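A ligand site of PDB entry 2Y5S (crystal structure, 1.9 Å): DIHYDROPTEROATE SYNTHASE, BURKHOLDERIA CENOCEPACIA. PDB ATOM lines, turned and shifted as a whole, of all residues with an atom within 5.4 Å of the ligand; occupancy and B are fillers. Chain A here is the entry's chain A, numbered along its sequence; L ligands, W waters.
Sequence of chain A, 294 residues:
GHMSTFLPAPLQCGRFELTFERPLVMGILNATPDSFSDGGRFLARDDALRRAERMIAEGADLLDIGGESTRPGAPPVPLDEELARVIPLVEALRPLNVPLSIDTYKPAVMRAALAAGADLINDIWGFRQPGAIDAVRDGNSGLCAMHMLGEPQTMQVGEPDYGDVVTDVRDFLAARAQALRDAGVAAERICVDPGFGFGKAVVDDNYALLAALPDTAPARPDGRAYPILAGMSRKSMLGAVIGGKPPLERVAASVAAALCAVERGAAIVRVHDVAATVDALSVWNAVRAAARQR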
ATOM      1  N   ASP A  64     -37.065 -24.513  -2.924  1.00  0.00           N
ATOM      2  CA  ASP A  64     -35.615 -24.606  -3.041  1.00  0.00           C
ATOM      3  C   ASP A  64     -35.010 -24.310  -1.699  1.00  0.00           C
ATOM      4  O   ASP A  64     -35.076 -23.195  -1.224  1.00  0.00           O
ATOM      5  CB  ASP A  64     -35.100 -23.612  -4.083  1.00  0.00           C
ATOM      6  CG  ASP A  64     -33.654 -23.908  -4.544  1.00  0.00           C
ATOM      7  OD1 ASP A  64     -33.219 -25.079  -4.532  1.00  0.00           O
ATOM      8  OD2 ASP A  64     -32.965 -22.951  -4.958  1.00  0.00           O
ATOM      9  N   THR A  70     -25.204 -19.168  -2.129  1.00  0.00           N
ATOM     10  CA  THR A  70     -24.781 -19.584  -3.466  1.00  0.00           C
ATOM     11  C   THR A  70     -24.907 -18.403  -4.441  1.00  0.00           C
ATOM     12  O   THR A  70     -25.786 -18.382  -5.316  1.00  0.00           O
ATOM     13  CB  THR A  70     -25.693 -20.718  -3.969  1.00  0.00           C
ATOM     14  OG1 THR A  70     -27.022 -20.443  -3.515  1.00  0.00           O
ATOM     15  CG2 THR A  70     -25.249 -22.081  -3.442  1.00  0.00           C
ATOM     16  N   ARG A  71     -24.044 -17.403  -4.277  1.00  0.00           N
ATOM     17  CA  ARG A  71     -24.102 -16.193  -5.099  1.00  0.00           C
ATOM     18  C   ARG A  71     -22.701 -15.579  -5.182  1.00  0.00           C
ATOM     19  O   ARG A  71     -21.896 -15.775  -4.270  1.00  0.00           O
ATOM     20  CB  ARG A  71     -25.097 -15.172  -4.528  1.00  0.00           C
ATOM     21  CG  ARG A  71     -24.688 -14.535  -3.179  1.00  0.00           C
ATOM     22  CD  ARG A  71     -25.476 -13.261  -2.876  1.00  0.00           C
ATOM     23  NE  ARG A  71     -25.185 -12.741  -1.535  1.00  0.00           N
ATOM     24  CZ  ARG A  71     -24.117 -12.014  -1.199  1.00  0.00           C
ATOM     25  NH1 ARG A  71     -23.189 -11.692  -2.098  1.00  0.00           N
ATOM     26  NH2 ARG A  71     -23.978 -11.602   0.055  1.00  0.00           N
ATOM     27  N   PRO A  72     -22.409 -14.834  -6.266  1.00  0.00           N
ATOM     28  CA  PRO A  72     -21.079 -14.226  -6.414  1.00  0.00           C
ATOM     29  C   PRO A  72     -20.667 -13.368  -5.206  1.00  0.00           C
ATOM     30  O   PRO A  72     -21.499 -12.636  -4.663  1.00  0.00           O
ATOM     31  CB  PRO A  72     -21.240 -13.335  -7.661  1.00  0.00           C
ATOM     32  CG  PRO A  72     -22.349 -13.954  -8.420  1.00  0.00           C
ATOM     33  CD  PRO A  72     -23.297 -14.455  -7.374  1.00  0.00           C
ATOM     34  N   ASP A 103     -30.354 -26.261  -3.123  1.00  0.00           N
ATOM     35  CA  ASP A 103     -29.430 -25.277  -3.724  1.00  0.00           C
ATOM     36  C   ASP A 103     -28.057 -25.478  -3.108  1.00  0.00           C
ATOM     37  O   ASP A 103     -27.729 -24.911  -2.046  1.00  0.00           O
ATOM     38  CB  ASP A 103     -29.944 -23.852  -3.470  1.00  0.00           C
ATOM     39  CG  ASP A 103     -29.018 -22.776  -4.029  1.00  0.00           C
ATOM     40  OD1 ASP A 103     -28.086 -23.084  -4.780  1.00  0.00           O
ATOM     41  OD2 ASP A 103     -29.222 -21.603  -3.700  1.00  0.00           O
ATOM     42  N   ASN A 122     -29.964 -28.581  -7.274  1.00  0.00           N
ATOM     43  CA  ASN A 122     -29.842 -27.347  -8.020  1.00  0.00           C
ATOM     44  C   ASN A 122     -28.435 -26.780  -7.789  1.00  0.00           C
ATOM     45  O   ASN A 122     -28.124 -26.277  -6.716  1.00  0.00           O
ATOM     46  CB  ASN A 122     -30.934 -26.359  -7.570  1.00  0.00           C
ATOM     47  CG  ASN A 122     -30.784 -25.007  -8.186  1.00  0.00           C
ATOM     48  OD1 ASN A 122     -30.296 -24.894  -9.303  1.00  0.00           O
ATOM     49  ND2 ASN A 122     -31.207 -23.973  -7.481  1.00  0.00           N
ATOM     50  N   ILE A 124     -25.290 -24.397  -8.787  1.00  0.00           N
ATOM     51  CA  ILE A 124     -24.699 -23.243  -9.435  1.00  0.00           C
ATOM     52  C   ILE A 124     -23.374 -23.525 -10.173  1.00  0.00           C
ATOM     53  O   ILE A 124     -23.015 -22.791 -11.090  1.00  0.00           O
ATOM     54  CB  ILE A 124     -24.502 -22.074  -8.466  1.00  0.00           C
ATOM     55  CG1 ILE A 124     -23.490 -22.411  -7.376  1.00  0.00           C
ATOM     56  CG2 ILE A 124     -25.876 -21.625  -7.896  1.00  0.00           C
ATOM     57  CD1 ILE A 124     -22.830 -21.142  -6.798  1.00  0.00           C
ATOM     58  N   CYS A 144     -30.598 -29.634 -11.866  1.00  0.00           N
ATOM     59  CA  CYS A 144     -30.462 -28.367 -12.559  1.00  0.00           C
ATOM     60  C   CYS A 144     -29.006 -27.965 -12.691  1.00  0.00           C
ATOM     61  O   CYS A 144     -28.347 -27.616 -11.715  1.00  0.00           O
ATOM     62  CB  CYS A 144     -31.248 -27.263 -11.888  1.00  0.00           C
ATOM     63  SG  CYS A 144     -31.150 -25.693 -12.828  1.00  0.00           S
ATOM     64  N   MET A 146     -26.715 -25.235 -13.829  1.00  0.00           N
ATOM     65  CA  MET A 146     -26.646 -23.809 -14.104  1.00  0.00           C
ATOM     66  C   MET A 146     -25.333 -23.400 -14.757  1.00  0.00           C
ATOM     67  O   MET A 146     -24.286 -24.022 -14.531  1.00  0.00           O
ATOM     68  CB  MET A 146     -26.848 -23.039 -12.794  1.00  0.00           C
ATOM     69  CG  MET A 146     -27.255 -21.581 -12.991  1.00  0.00           C
ATOM     70  SD  MET A 146     -27.077 -20.609 -11.476  1.00  0.00           S
ATOM     71  CE  MET A 146     -25.360 -20.133 -11.566  1.00  0.00           C
ATOM     72  N   ASP A 193     -30.183 -23.937 -16.704  1.00  0.00           N
ATOM     73  CA  ASP A 193     -30.400 -22.593 -16.223  1.00  0.00           C
ATOM     74  C   ASP A 193     -29.224 -21.717 -16.677  1.00  0.00           C
ATOM     75  O   ASP A 193     -28.056 -22.040 -16.390  1.00  0.00           O
ATOM     76  CB  ASP A 193     -30.517 -22.683 -14.701  1.00  0.00           C
ATOM     77  CG  ASP A 193     -30.711 -21.335 -14.019  1.00  0.00           C
ATOM     78  OD1 ASP A 193     -30.437 -20.270 -14.601  1.00  0.00           O
ATOM     79  OD2 ASP A 193     -31.121 -21.376 -12.839  1.00  0.00           O
ATOM     80  N   GLY A 195     -28.209 -18.998 -15.527  1.00  0.00           N
ATOM     81  CA  GLY A 195     -27.502 -18.386 -14.396  1.00  0.00           C
ATOM     82  C   GLY A 195     -27.436 -16.876 -14.435  1.00  0.00           C
ATOM     83  O   GLY A 195     -26.348 -16.278 -14.467  1.00  0.00           O
ATOM     84  N   PHE A 196     -28.593 -16.246 -14.426  1.00  0.00           N
ATOM     85  CA  PHE A 196     -28.666 -14.802 -14.386  1.00  0.00           C
ATOM     86  C   PHE A 196     -27.866 -14.283 -13.207  1.00  0.00           C
ATOM     87  O   PHE A 196     -27.992 -14.794 -12.089  1.00  0.00           O
ATOM     88  CB  PHE A 196     -30.123 -14.343 -14.334  1.00  0.00           C
ATOM     89  CG  PHE A 196     -30.886 -14.613 -15.599  1.00  0.00           C
ATOM     90  CD1 PHE A 196     -30.744 -13.785 -16.690  1.00  0.00           C
ATOM     91  CD2 PHE A 196     -31.774 -15.679 -15.689  1.00  0.00           C
ATOM     92  CE1 PHE A 196     -31.437 -14.041 -17.871  1.00  0.00           C
ATOM     93  CE2 PHE A 196     -32.501 -15.920 -16.867  1.00  0.00           C
ATOM     94  CZ  PHE A 196     -32.327 -15.100 -17.942  1.00  0.00           C
ATOM     95  N   GLY A 197     -26.968 -13.340 -13.487  1.00  0.00           N
ATOM     96  CA  GLY A 197     -26.189 -12.638 -12.479  1.00  0.00           C
ATOM     97  C   GLY A 197     -24.934 -13.353 -12.007  1.00  0.00           C
ATOM     98  O   GLY A 197     -24.300 -12.890 -11.061  1.00  0.00           O
ATOM     99  N   PHE A 198     -24.567 -14.455 -12.660  1.00  0.00           N
ATOM    100  CA  PHE A 198     -23.339 -15.202 -12.348  1.00  0.00           C
ATOM    101  C   PHE A 198     -22.299 -15.087 -13.465  1.00  0.00           C
ATOM    102  O   PHE A 198     -22.262 -15.913 -14.382  1.00  0.00           O
ATOM    103  CB  PHE A 198     -23.635 -16.668 -12.135  1.00  0.00           C
ATOM    104  CG  PHE A 198     -24.448 -16.974 -10.906  1.00  0.00           C
ATOM    105  CD1 PHE A 198     -25.838 -16.985 -10.961  1.00  0.00           C
ATOM    106  CD2 PHE A 198     -23.815 -17.348  -9.719  1.00  0.00           C
ATOM    107  CE1 PHE A 198     -26.594 -17.327  -9.864  1.00  0.00           C
ATOM    108  CE2 PHE A 198     -24.549 -17.698  -8.597  1.00  0.00           C
ATOM    109  CZ  PHE A 198     -25.950 -17.701  -8.655  1.00  0.00           C
ATOM    110  N   LEU A 229     -34.899 -23.641 -16.144  1.00  0.00           N
ATOM    111  CA  LEU A 229     -35.185 -22.964 -14.891  1.00  0.00           C
ATOM    112  C   LEU A 229     -34.508 -21.592 -14.964  1.00  0.00           C
ATOM    113  O   LEU A 229     -33.364 -21.479 -15.405  1.00  0.00           O
ATOM    114  CB  LEU A 229     -34.661 -23.788 -13.711  1.00  0.00           C
ATOM    115  CG  LEU A 229     -35.011 -23.322 -12.282  1.00  0.00           C
ATOM    116  CD1 LEU A 229     -34.967 -24.551 -11.358  1.00  0.00           C
ATOM    117  CD2 LEU A 229     -34.094 -22.254 -11.755  1.00  0.00           C
ATOM    118  N   ALA A 230     -35.227 -20.540 -14.569  1.00  0.00           N
ATOM    119  CA  ALA A 230     -34.688 -19.184 -14.601  1.00  0.00           C
ATOM    120  C   ALA A 230     -34.895 -18.533 -13.228  1.00  0.00           C
ATOM    121  O   ALA A 230     -35.960 -18.619 -12.643  1.00  0.00           O
ATOM    122  CB  ALA A 230     -35.363 -18.367 -15.681  1.00  0.00           C
ATOM    123  N   GLY A 231     -33.845 -17.897 -12.713  1.00  0.00           N
ATOM    124  CA  GLY A 231     -33.927 -17.218 -11.428  1.00  0.00           C
ATOM    125  C   GLY A 231     -33.432 -15.811 -11.565  1.00  0.00           C
ATOM    126  O   GLY A 231     -32.242 -15.603 -11.772  1.00  0.00           O
ATOM    127  N   MET A 232     -34.343 -14.840 -11.482  1.00  0.00           N
ATOM    128  CA  MET A 232     -33.985 -13.409 -11.530  1.00  0.00           C
ATOM    129  C   MET A 232     -34.457 -12.583 -10.351  1.00  0.00           C
ATOM    130  O   MET A 232     -34.182 -11.374 -10.272  1.00  0.00           O
ATOM    131  CB  MET A 232     -34.544 -12.811 -12.802  1.00  0.00           C
ATOM    132  CG  MET A 232     -33.805 -13.309 -14.018  1.00  0.00           C
ATOM    133  SD  MET A 232     -34.605 -12.852 -15.530  1.00  0.00           S
ATOM    134  CE  MET A 232     -35.933 -14.002 -15.467  1.00  0.00           C
ATOM    135  N   ARG A 234     -35.288 -10.414  -7.478  1.00  0.00           N
ATOM    136  CA  ARG A 234     -34.613  -9.392  -6.663  1.00  0.00           C
ATOM    137  C   ARG A 234     -33.140  -9.133  -7.020  1.00  0.00           C
ATOM    138  O   ARG A 234     -32.421  -8.510  -6.253  1.00  0.00           O
ATOM    139  CB  ARG A 234     -34.740  -9.724  -5.173  1.00  0.00           C
ATOM    140  CG  ARG A 234     -36.177  -9.756  -4.692  1.00  0.00           C
ATOM    141  CD  ARG A 234     -36.260 -10.057  -3.200  1.00  0.00           C
ATOM    142  NE  ARG A 234     -37.649 -10.023  -2.718  1.00  0.00           N
ATOM    143  CZ  ARG A 234     -38.016 -10.308  -1.460  1.00  0.00           C
ATOM    144  NH1 ARG A 234     -37.100 -10.643  -0.547  1.00  0.00           N
ATOM    145  NH2 ARG A 234     -39.297 -10.265  -1.103  1.00  0.00           N
ATOM    146  N   LYS A 235     -32.709  -9.573  -8.189  1.00  0.00           N
ATOM    147  CA  LYS A 235     -31.284  -9.524  -8.527  1.00  0.00           C
ATOM    148  C   LYS A 235     -30.887  -8.169  -9.045  1.00  0.00           C
ATOM    149  O   LYS A 235     -31.745  -7.342  -9.418  1.00  0.00           O
ATOM    150  CB  LYS A 235     -30.948 -10.609  -9.560  1.00  0.00           C
ATOM    151  CG  LYS A 235     -30.938 -11.996  -8.986  1.00  0.00           C
ATOM    152  CD  LYS A 235     -30.287 -13.015  -9.938  1.00  0.00           C
ATOM    153  CE  LYS A 235     -30.270 -14.434  -9.310  1.00  0.00           C
ATOM    154  NZ  LYS A 235     -29.930 -15.489 -10.321  1.00  0.00           N
ATOM    155  N   SER A 236     -29.573  -7.954  -9.099  1.00  0.00           N
ATOM    156  CA  SER A 236     -28.957  -6.713  -9.585  1.00  0.00           C
ATOM    157  C   SER A 236     -29.382  -6.277 -10.963  1.00  0.00           C
ATOM    158  O   SER A 236     -29.530  -5.078 -11.224  1.00  0.00           O
ATOM    159  CB  SER A 236     -27.429  -6.878  -9.588  1.00  0.00           C
ATOM    160  OG  SER A 236     -26.998  -6.820  -8.257  1.00  0.00           O
ATOM    161  N   MET A 237     -29.562  -7.233 -11.868  1.00  0.00           N
ATOM    162  CA  MET A 237     -30.047  -6.893 -13.205  1.00  0.00           C
ATOM    163  C   MET A 237     -31.344  -6.082 -13.151  1.00  0.00           C
ATOM    164  O   MET A 237     -31.605  -5.271 -14.046  1.00  0.00           O
ATOM    165  CB  MET A 237     -30.234  -8.151 -14.068  1.00  0.00           C
ATOM    166  CG  MET A 237     -31.231  -9.181 -13.519  1.00  0.00           C
ATOM    167  SD  MET A 237     -31.434 -10.622 -14.605  1.00  0.00           S
ATOM    168  CE  MET A 237     -32.349  -9.947 -15.988  1.00  0.00           C
ATOM    169  N   ARG A 250     -37.683  -4.520  -5.252  1.00  0.00           N
ATOM    170  CA  ARG A 250     -37.581  -5.016  -6.611  1.00  0.00           C
ATOM    171  C   ARG A 250     -38.693  -6.013  -6.918  1.00  0.00           C
ATOM    172  O   ARG A 250     -38.571  -6.809  -7.863  1.00  0.00           O
ATOM    173  CB  ARG A 250     -36.207  -5.677  -6.841  1.00  0.00           C
ATOM    174  CG  ARG A 250     -35.010  -4.719  -6.813  1.00  0.00           C
ATOM    175  CD  ARG A 250     -33.660  -5.445  -6.936  1.00  0.00           C
ATOM    176  NE  ARG A 250     -32.579  -4.540  -6.598  1.00  0.00           N
ATOM    177  CZ  ARG A 250     -31.310  -4.859  -6.328  1.00  0.00           C
ATOM    178  NH1 ARG A 250     -30.889  -6.111  -6.351  1.00  0.00           N
ATOM    179  NH2 ARG A 250     -30.465  -3.901  -6.001  1.00  0.00           N
ATOM    180  N   ARG A 270     -37.790 -19.248 -10.403  1.00  0.00           N
ATOM    181  CA  ARG A 270     -37.349 -19.332  -9.021  1.00  0.00           C
ATOM    182  C   ARG A 270     -37.480 -17.951  -8.432  1.00  0.00           C
ATOM    183  O   ARG A 270     -36.860 -17.020  -8.937  1.00  0.00           O
ATOM    184  CB  ARG A 270     -35.892 -19.832  -9.006  1.00  0.00           C
ATOM    185  CG  ARG A 270     -35.273 -20.033  -7.636  1.00  0.00           C
ATOM    186  CD  ARG A 270     -33.810 -20.525  -7.782  1.00  0.00           C
ATOM    187  NE  ARG A 270     -33.193 -20.670  -6.465  1.00  0.00           N
ATOM    188  CZ  ARG A 270     -32.633 -19.688  -5.748  1.00  0.00           C
ATOM    189  NH1 ARG A 270     -32.591 -18.436  -6.187  1.00  0.00           N
ATOM    190  NH2 ARG A 270     -32.133 -19.967  -4.549  1.00  0.00           N
HETATM  191  O1  LIG L   1     -30.518 -17.974 -10.552  1.00  0.00           O
HETATM  192  C1  LIG L   1     -30.363 -19.031  -9.937  1.00  0.00           C
HETATM  193  C2  LIG L   1     -29.921 -19.025  -8.608  1.00  0.00           C
HETATM  194  N1  LIG L   1     -30.632 -20.266 -10.569  1.00  0.00           N
HETATM  195  C3  LIG L   1     -29.749 -20.256  -7.974  1.00  0.00           C
HETATM  196  N2  LIG L   1     -29.687 -17.865  -7.952  1.00  0.00           N
HETATM  197  C4  LIG L   1     -30.404 -21.467  -9.857  1.00  0.00           C
HETATM  198  N3  LIG L   1     -29.320 -20.289  -6.653  1.00  0.00           N
HETATM  199  N4  LIG L   1     -30.003 -21.417  -8.588  1.00  0.00           N
HETATM  200  C5  LIG L   1     -29.117 -17.844  -6.748  1.00  0.00           C
HETATM  201  N5  LIG L   1     -30.609 -22.662 -10.446  1.00  0.00           N
HETATM  202  C6  LIG L   1     -28.645 -19.135  -6.043  1.00  0.00           C
HETATM  203  C7  LIG L   1     -28.937 -16.519  -6.026  1.00  0.00           C
HETATM  204  N6  LIG L   1     -27.675 -15.905  -6.414  1.00  0.00           N
HETATM  205  C8  LIG L   1     -27.634 -14.647  -6.833  1.00  0.00           C
HETATM  206  C9  LIG L   1     -28.279 -13.669  -6.089  1.00  0.00           C
HETATM  207  C10 LIG L   1     -26.955 -14.332  -8.020  1.00  0.00           C
HETATM  208  C11 LIG L   1     -28.231 -12.348  -6.519  1.00  0.00           C
HETATM  209  C12 LIG L   1     -26.925 -13.025  -8.447  1.00  0.00           C
HETATM  210  C13 LIG L   1     -27.563 -12.033  -7.696  1.00  0.00           C
HETATM  211  C14 LIG L   1     -27.534 -10.578  -8.196  1.00  0.00           C
HETATM  212  O2  LIG L   1     -27.159 -10.377  -9.360  1.00  0.00           O
HETATM  213  O3  LIG L   1     -27.949  -9.678  -7.443  1.00  0.00           O
HETATM  214  O   HOH W   1     -28.180  -9.858 -11.672  1.00  0.00           O
HETATM  215  O   HOH W   2     -24.339 -10.657 -10.013  1.00  0.00           O
HETATM  216  O   HOH W   3     -30.977 -17.969 -13.330  1.00  0.00           O
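The side-chain amide oxygen of Asn 122 is in hydrogen-bond range of a nitrogen (N5) of the ligand, 2.5 Å away.
An oxygen (O1) of the ligand lies within hydrogen-bond range of the side-chain amino group (NZ) of Lys 235, 2.6 Å away.
The side-chain carboxylate (OD2) of Asp 193 sits at hydrogen-bond distance from a nitrogen (N1) of the ligand (2.6 Å).
O3 of the ligand sits at hydrogen-bond distance from N of Ser 236, at 2.9 Å.
O3 of the ligand sits at hydrogen-bond distance from OG of Ser 236.
A nitrogen (N6) of the ligand sits close to the backbone carbonyl oxygen (O) of Thr 70 (3.3 Å).
A nitrogen (N3) of the ligand lies within hydrogen-bond range of the side-chain carboxylate (OD2) of Asp 103, at 3.2 Å.
NH1 of Arg 270 is in hydrogen-bond range of N2 of the ligand (3.4 Å).
A nitrogen (N1) of the ligand sits at hydrogen-bond distance from the side-chain sulfur (SD) of Met 146, at 3.7 Å.
The side-chain amide oxygen of Asn 122 lies close to the side-chain sulfur of Cys 144 (3.7 Å).
NZ of Lys 235 is in hydrogen-bond range of O of Gly 231, 2.7 Å away.
O of Phe 196 is in hydrogen-bond range of NZ of Lys 235.
OD1 of Asp 193 sits at hydrogen-bond distance from N of Gly 195 (2.7 Å).
The side-chain carboxylate (OD2) of Asp 103 lies within hydrogen-bond range of the side-chain hydroxyl (OG1) of Thr 70 (2.5 Å).
The side-chain carboxylate (OD2) of Asp 103 is in salt-bridge range of the guanidinium group (NH2) of Arg 270 (3.4 Å).
The backbone NH of Asp 103 is in hydrogen-bond range of the side-chain carboxylate of Asp 64 (3.4 Å).
OD2 of Asp 64 lies within salt-bridge range of NE of Arg 270 (2.7 Å).
The backbone carbonyl oxygen of Gly 231 sits close to an oxygen (O1) of the ligand, 3.2 Å away.
Residues that only touch the ligand: Arg 71 (3.3 Å), Pro 72 (3.7 Å), Ile 124 (3.9 Å), Cys 144 (3.9 Å), Gly 197 (3.7 Å), Phe 198 (3.4 Å) and Leu 229 (3.7 Å).
Within 4 Å of the ligand: Thr 70, Arg 71, Pro 72, Asp 103, Asn 122, Ile 124, Cys 144, Met 146, Asp 193, Gly 197, Phe 198, Leu 229, Gly 231, Lys 235, Ser 236 and Arg 270.
The nearest printed residue that does not touch the ligand is Phe 196 (4.2 Å).
Water W1 lies within hydrogen-bond range of O2 of the ligand (2.6 Å), N of Met 237 (3.0 Å) and N of Ser 236 (3.5 Å).
Water W3 lies within hydrogen-bond range of the side-chain carboxylate (OD1) of Asp 193 (2.7 Å), an oxygen (O1) of the ligand (2.8 Å), the backbone NH (N) of Gly 231 (2.9 Å) and the backbone NH (N) of Phe 196 (3.1 Å).
Water W2 bridges O of Gly 197 (2.5 Å) and O2 of the ligand (2.9 Å).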
